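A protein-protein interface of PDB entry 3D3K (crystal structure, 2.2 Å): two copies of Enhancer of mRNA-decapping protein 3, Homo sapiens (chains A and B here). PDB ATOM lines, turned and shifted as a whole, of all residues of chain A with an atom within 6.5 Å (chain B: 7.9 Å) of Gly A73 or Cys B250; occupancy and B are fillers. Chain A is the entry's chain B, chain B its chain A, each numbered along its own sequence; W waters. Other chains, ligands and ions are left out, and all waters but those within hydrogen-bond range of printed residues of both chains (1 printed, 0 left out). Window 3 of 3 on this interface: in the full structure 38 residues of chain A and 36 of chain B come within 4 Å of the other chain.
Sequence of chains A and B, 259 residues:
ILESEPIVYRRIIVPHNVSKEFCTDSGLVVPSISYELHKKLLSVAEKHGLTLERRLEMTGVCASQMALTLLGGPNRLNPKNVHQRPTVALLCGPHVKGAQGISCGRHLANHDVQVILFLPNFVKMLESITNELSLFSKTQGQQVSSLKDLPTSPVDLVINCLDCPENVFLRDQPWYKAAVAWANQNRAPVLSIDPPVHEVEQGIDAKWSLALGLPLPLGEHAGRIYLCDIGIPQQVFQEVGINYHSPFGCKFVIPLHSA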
ATOM      1  N   GLN A  65      18.649  27.001   3.732  1.00  0.00           N
ATOM      2  CA  GLN A  65      20.061  27.166   3.355  1.00  0.00           C
ATOM      3  C   GLN A  65      20.211  28.284   2.339  1.00  0.00           C
ATOM      4  O   GLN A  65      21.104  29.118   2.466  1.00  0.00           O
ATOM      5  CB  GLN A  65      20.643  25.866   2.787  1.00  0.00           C
ATOM      6  CG  GLN A  65      20.914  24.798   3.855  1.00  0.00           C
ATOM      7  CD  GLN A  65      21.508  23.501   3.310  1.00  0.00           C
ATOM      8  OE1 GLN A  65      21.285  23.122   2.167  1.00  0.00           O
ATOM      9  NE2 GLN A  65      22.250  22.805   4.152  1.00  0.00           N
ATOM     10  N   ALA A  67      17.925  30.727   1.868  1.00  0.00           N
ATOM     11  CA  ALA A  67      17.562  31.950   2.605  1.00  0.00           C
ATOM     12  C   ALA A  67      18.702  32.503   3.484  1.00  0.00           C
ATOM     13  O   ALA A  67      18.875  33.722   3.586  1.00  0.00           O
ATOM     14  CB  ALA A  67      16.292  31.734   3.433  1.00  0.00           C
ATOM     15  N   LEU A  68      19.477  31.606   4.102  1.00  0.00           N
ATOM     16  CA  LEU A  68      20.600  31.999   4.962  1.00  0.00           C
ATOM     17  C   LEU A  68      21.735  32.652   4.176  1.00  0.00           C
ATOM     18  O   LEU A  68      22.434  33.521   4.696  1.00  0.00           O
ATOM     19  CB  LEU A  68      21.132  30.801   5.771  1.00  0.00           C
ATOM     20  CG  LEU A  68      20.288  30.332   6.970  1.00  0.00           C
ATOM     21  CD1 LEU A  68      20.588  28.879   7.350  1.00  0.00           C
ATOM     22  CD2 LEU A  68      20.468  31.255   8.172  1.00  0.00           C
ATOM     23  N   THR A  69      21.910  32.224   2.928  1.00  0.00           N
ATOM     24  CA  THR A  69      22.856  32.859   2.011  1.00  0.00           C
ATOM     25  C   THR A  69      22.385  34.274   1.635  1.00  0.00           C
ATOM     26  O   THR A  69      23.194  35.198   1.500  1.00  0.00           O
ATOM     27  CB  THR A  69      23.056  32.013   0.728  1.00  0.00           C
ATOM     28  OG1 THR A  69      23.583  30.723   1.080  1.00  0.00           O
ATOM     29  CG2 THR A  69      24.032  32.698  -0.223  1.00  0.00           C
ATOM     30  N   LEU A  70      21.076  34.434   1.465  1.00  0.00           N
ATOM     31  CA  LEU A  70      20.516  35.722   1.097  1.00  0.00           C
ATOM     32  C   LEU A  70      20.616  36.667   2.280  1.00  0.00           C
ATOM     33  O   LEU A  70      20.687  37.880   2.104  1.00  0.00           O
ATOM     34  CB  LEU A  70      19.059  35.579   0.641  1.00  0.00           C
ATOM     35  CG  LEU A  70      18.721  34.654  -0.535  1.00  0.00           C
ATOM     36  CD1 LEU A  70      17.236  34.717  -0.796  1.00  0.00           C
ATOM     37  CD2 LEU A  70      19.508  35.003  -1.805  1.00  0.00           C
ATOM     38  N   LEU A  71      20.639  36.097   3.482  1.00  0.00           N
ATOM     39  CA  LEU A  71      20.736  36.865   4.711  1.00  0.00           C
ATOM     40  C   LEU A  71      22.180  37.229   5.063  1.00  0.00           C
ATOM     41  O   LEU A  71      22.426  37.878   6.078  1.00  0.00           O
ATOM     42  CB  LEU A  71      20.063  36.115   5.874  1.00  0.00           C
ATOM     43  CG  LEU A  71      18.543  35.945   5.804  1.00  0.00           C
ATOM     44  CD1 LEU A  71      18.056  34.960   6.860  1.00  0.00           C
ATOM     45  CD2 LEU A  71      17.835  37.276   5.929  1.00  0.00           C
ATOM     46  N   GLY A  72      23.127  36.810   4.223  1.00  0.00           N
ATOM     47  CA  GLY A  72      24.531  37.204   4.378  1.00  0.00           C
ATOM     48  C   GLY A  72      25.463  36.111   4.870  1.00  0.00           C
ATOM     49  O   GLY A  72      26.689  36.251   4.773  1.00  0.00           O
ATOM     50  N   GLY A  73      24.880  35.037   5.409  1.00  0.00           N
ATOM     51  CA  GLY A  73      25.616  33.871   5.924  1.00  0.00           C
ATOM     52  C   GLY A  73      26.885  34.151   6.721  1.00  0.00           C
ATOM     53  O   GLY A  73      27.979  33.786   6.273  1.00  0.00           O
ATOM     54  N   PRO A  74      26.752  34.765   7.919  1.00  0.00           N
ATOM     55  CA  PRO A  74      27.927  35.229   8.687  1.00  0.00           C
ATOM     56  C   PRO A  74      28.882  34.101   9.081  1.00  0.00           C
ATOM     57  O   PRO A  74      29.996  34.020   8.551  1.00  0.00           O
ATOM     58  CB  PRO A  74      27.308  35.861   9.946  1.00  0.00           C
ATOM     59  CG  PRO A  74      25.884  36.153   9.576  1.00  0.00           C
ATOM     60  CD  PRO A  74      25.495  35.040   8.640  1.00  0.00           C
ATOM     61  N   HIS A 111      18.137  27.950  13.365  1.00  0.00           N
ATOM     62  CA  HIS A 111      19.425  28.579  13.122  1.00  0.00           C
ATOM     63  C   HIS A 111      19.471  30.044  13.550  1.00  0.00           C
ATOM     64  O   HIS A 111      20.199  30.857  12.968  1.00  0.00           O
ATOM     65  CB  HIS A 111      19.838  28.380  11.663  1.00  0.00           C
ATOM     66  CG  HIS A 111      20.255  26.975  11.363  1.00  0.00           C
ATOM     67  ND1 HIS A 111      21.575  26.580  11.339  1.00  0.00           N
ATOM     68  CD2 HIS A 111      19.525  25.862  11.109  1.00  0.00           C
ATOM     69  CE1 HIS A 111      21.642  25.290  11.070  1.00  0.00           C
ATOM     70  NE2 HIS A 111      20.411  24.829  10.931  1.00  0.00           N
ATOM     71  N   SER B 246      21.465  26.898  19.831  1.00  0.00           N
ATOM     72  CA  SER B 246      22.107  26.353  18.643  1.00  0.00           C
ATOM     73  C   SER B 246      23.593  26.709  18.525  1.00  0.00           C
ATOM     74  O   SER B 246      23.958  27.887  18.613  1.00  0.00           O
ATOM     75  CB  SER B 246      21.350  26.787  17.386  1.00  0.00           C
ATOM     76  OG  SER B 246      22.101  26.503  16.223  1.00  0.00           O
ATOM     77  N   PRO B 247      24.451  25.680  18.335  1.00  0.00           N
ATOM     78  CA  PRO B 247      25.881  25.835  18.081  1.00  0.00           C
ATOM     79  C   PRO B 247      26.235  25.928  16.591  1.00  0.00           C
ATOM     80  O   PRO B 247      27.413  26.048  16.245  1.00  0.00           O
ATOM     81  CB  PRO B 247      26.469  24.549  18.670  1.00  0.00           C
ATOM     82  CG  PRO B 247      25.403  23.527  18.465  1.00  0.00           C
ATOM     83  CD  PRO B 247      24.067  24.256  18.392  1.00  0.00           C
ATOM     84  N   PHE B 248      25.225  25.907  15.727  1.00  0.00           N
ATOM     85  CA  PHE B 248      25.441  25.732  14.292  1.00  0.00           C
ATOM     86  C   PHE B 248      25.793  26.996  13.502  1.00  0.00           C
ATOM     87  O   PHE B 248      26.449  26.905  12.461  1.00  0.00           O
ATOM     88  CB  PHE B 248      24.220  25.067  13.645  1.00  0.00           C
ATOM     89  CG  PHE B 248      23.993  23.656  14.091  1.00  0.00           C
ATOM     90  CD1 PHE B 248      24.844  22.640  13.678  1.00  0.00           C
ATOM     91  CD2 PHE B 248      22.919  23.342  14.919  1.00  0.00           C
ATOM     92  CE1 PHE B 248      24.649  21.331  14.095  1.00  0.00           C
ATOM     93  CE2 PHE B 248      22.706  22.031  15.343  1.00  0.00           C
ATOM     94  CZ  PHE B 248      23.588  21.025  14.933  1.00  0.00           C
ATOM     95  N   GLY B 249      25.353  28.159  13.980  1.00  0.00           N
ATOM     96  CA  GLY B 249      25.329  29.355  13.139  1.00  0.00           C
ATOM     97  C   GLY B 249      24.490  29.061  11.894  1.00  0.00           C
ATOM     98  O   GLY B 249      23.411  28.471  11.990  1.00  0.00           O
ATOM     99  N   CYS B 250      25.005  29.434  10.727  1.00  0.00           N
ATOM    100  CA  CYS B 250      24.307  29.226   9.455  1.00  0.00           C
ATOM    101  C   CYS B 250      24.566  27.863   8.795  1.00  0.00           C
ATOM    102  O   CYS B 250      24.004  27.575   7.736  1.00  0.00           O
ATOM    103  CB  CYS B 250      24.651  30.364   8.482  1.00  0.00           C
ATOM    104  SG  CYS B 250      26.414  30.475   8.069  1.00  0.00           S
ATOM    105  N   LYS B 251      25.399  27.027   9.418  1.00  0.00           N
ATOM    106  CA  LYS B 251      25.771  25.731   8.855  1.00  0.00           C
ATOM    107  C   LYS B 251      24.940  24.585   9.443  1.00  0.00           C
ATOM    108  O   LYS B 251      24.504  24.656  10.592  1.00  0.00           O
ATOM    109  CB  LYS B 251      27.268  25.464   9.058  1.00  0.00           C
ATOM    110  CG  LYS B 251      28.183  26.504   8.399  1.00  0.00           C
ATOM    111  CD  LYS B 251      29.596  25.976   8.209  1.00  0.00           C
ATOM    112  CE  LYS B 251      30.478  27.045   7.555  1.00  0.00           C
ATOM    113  NZ  LYS B 251      31.836  26.526   7.218  1.00  0.00           N
ATOM    114  N   PHE B 252      24.730  23.536   8.648  1.00  0.00           N
ATOM    115  CA  PHE B 252      23.949  22.372   9.071  1.00  0.00           C
ATOM    116  C   PHE B 252      24.845  21.225   9.546  1.00  0.00           C
ATOM    117  O   PHE B 252      24.383  20.312  10.235  1.00  0.00           O
ATOM    118  CB  PHE B 252      22.987  21.925   7.954  1.00  0.00           C
ATOM    119  CG  PHE B 252      21.724  22.761   7.867  1.00  0.00           C
ATOM    120  CD1 PHE B 252      20.490  22.217   8.218  1.00  0.00           C
ATOM    121  CD2 PHE B 252      21.776  24.099   7.466  1.00  0.00           C
ATOM    122  CE1 PHE B 252      19.322  22.994   8.151  1.00  0.00           C
ATOM    123  CE2 PHE B 252      20.630  24.876   7.397  1.00  0.00           C
ATOM    124  CZ  PHE B 252      19.394  24.322   7.747  1.00  0.00           C
ATOM    125  N   VAL B 253      26.124  21.291   9.167  1.00  0.00           N
ATOM    126  CA  VAL B 253      27.158  20.386   9.666  1.00  0.00           C
ATOM    127  C   VAL B 253      28.368  21.218  10.078  1.00  0.00           C
ATOM    128  O   VAL B 253      28.860  22.026   9.286  1.00  0.00           O
ATOM    129  CB  VAL B 253      27.599  19.328   8.608  1.00  0.00           C
ATOM    130  CG1 VAL B 253      28.745  18.482   9.149  1.00  0.00           C
ATOM    131  CG2 VAL B 253      26.424  18.438   8.198  1.00  0.00           C
ATOM    132  N   ILE B 254      28.827  21.025  11.316  1.00  0.00           N
ATOM    133  CA  ILE B 254      29.927  21.811  11.877  1.00  0.00           C
ATOM    134  C   ILE B 254      31.036  20.920  12.461  1.00  0.00           C
ATOM    135  O   ILE B 254      30.748  19.858  13.018  1.00  0.00           O
ATOM    136  CB  ILE B 254      29.427  22.823  12.954  1.00  0.00           C
ATOM    137  CG1 ILE B 254      28.665  22.100  14.075  1.00  0.00           C
ATOM    138  CG2 ILE B 254      28.552  23.906  12.298  1.00  0.00           C
ATOM    139  CD1 ILE B 254      28.530  22.887  15.357  1.00  0.00           C
HETATM  140  O   HOH W   1      25.111  23.878   5.647  1.00  0.00           O
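ND1 of His A111 is in hydrogen-bond range of O of Gly B249 (2.7 Å).
OG of Ser B246 is in hydrogen-bond range of N of Phe B248.
O of Gln A65 is in hydrogen-bond range of OG1 of Thr A69 (3.3 Å).
O of Leu A68 sits at hydrogen-bond distance from N of Gly A73, at 3.0 Å.
Among the printed residues, merely in contact across the chains: His A111 with Lys B251 (3.0 Å), His A111 with Phe B252 (3.4 Å), Gln A65 with Phe B252 (3.6 Å), His A111 with Phe B248 (3.7 Å), Leu A68 with Cys B250 (3.7 Å) and Gly A73 with Cys B250 (3.9 Å).
Of chain B, only Cys B250 comes within 4 Å of Gly A73.
No residue of chain B comes within 4 Å of Pro A74.
Of the printed residues of chain B, Gln A65 touches Phe B252 (3.6 Å).
Of the printed residues of chain A, Phe B252 touches Gln A65 (3.6 Å) and His A111 (3.4 Å).
Printed residues of chain B within 4 Å of His A111: Phe B248, Gly B249, Lys B251 and Phe B252.
Printed residues of chain A within 4 Å of Gly B249: His A111 (2.7 Å).
Ala A67 touches none of the printed residues of chain B.
Ser B246 touches none of the printed residues of chain A.
The nearest residue of chain A that does not touch Cys B250 is His A111 (4.1 Å).
The nearest printed residue of chain B that does not touch Gln A65 is Cys B250 (5.7 Å).
Of the 9 printed residues of chain B, 5 touch a printed residue of chain A.
Hydrophobic or aromatic side chains of chain B within 4 Å of the printed part of chain A: Phe B248 and Phe B252.
No position is printed for both chains.
Water W1 lies within hydrogen-bond range of the backbone NH (N) of Phe B252 (3.0 Å) and the side-chain amide nitrogen (NE2) of Gln A65 (3.4 Å).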
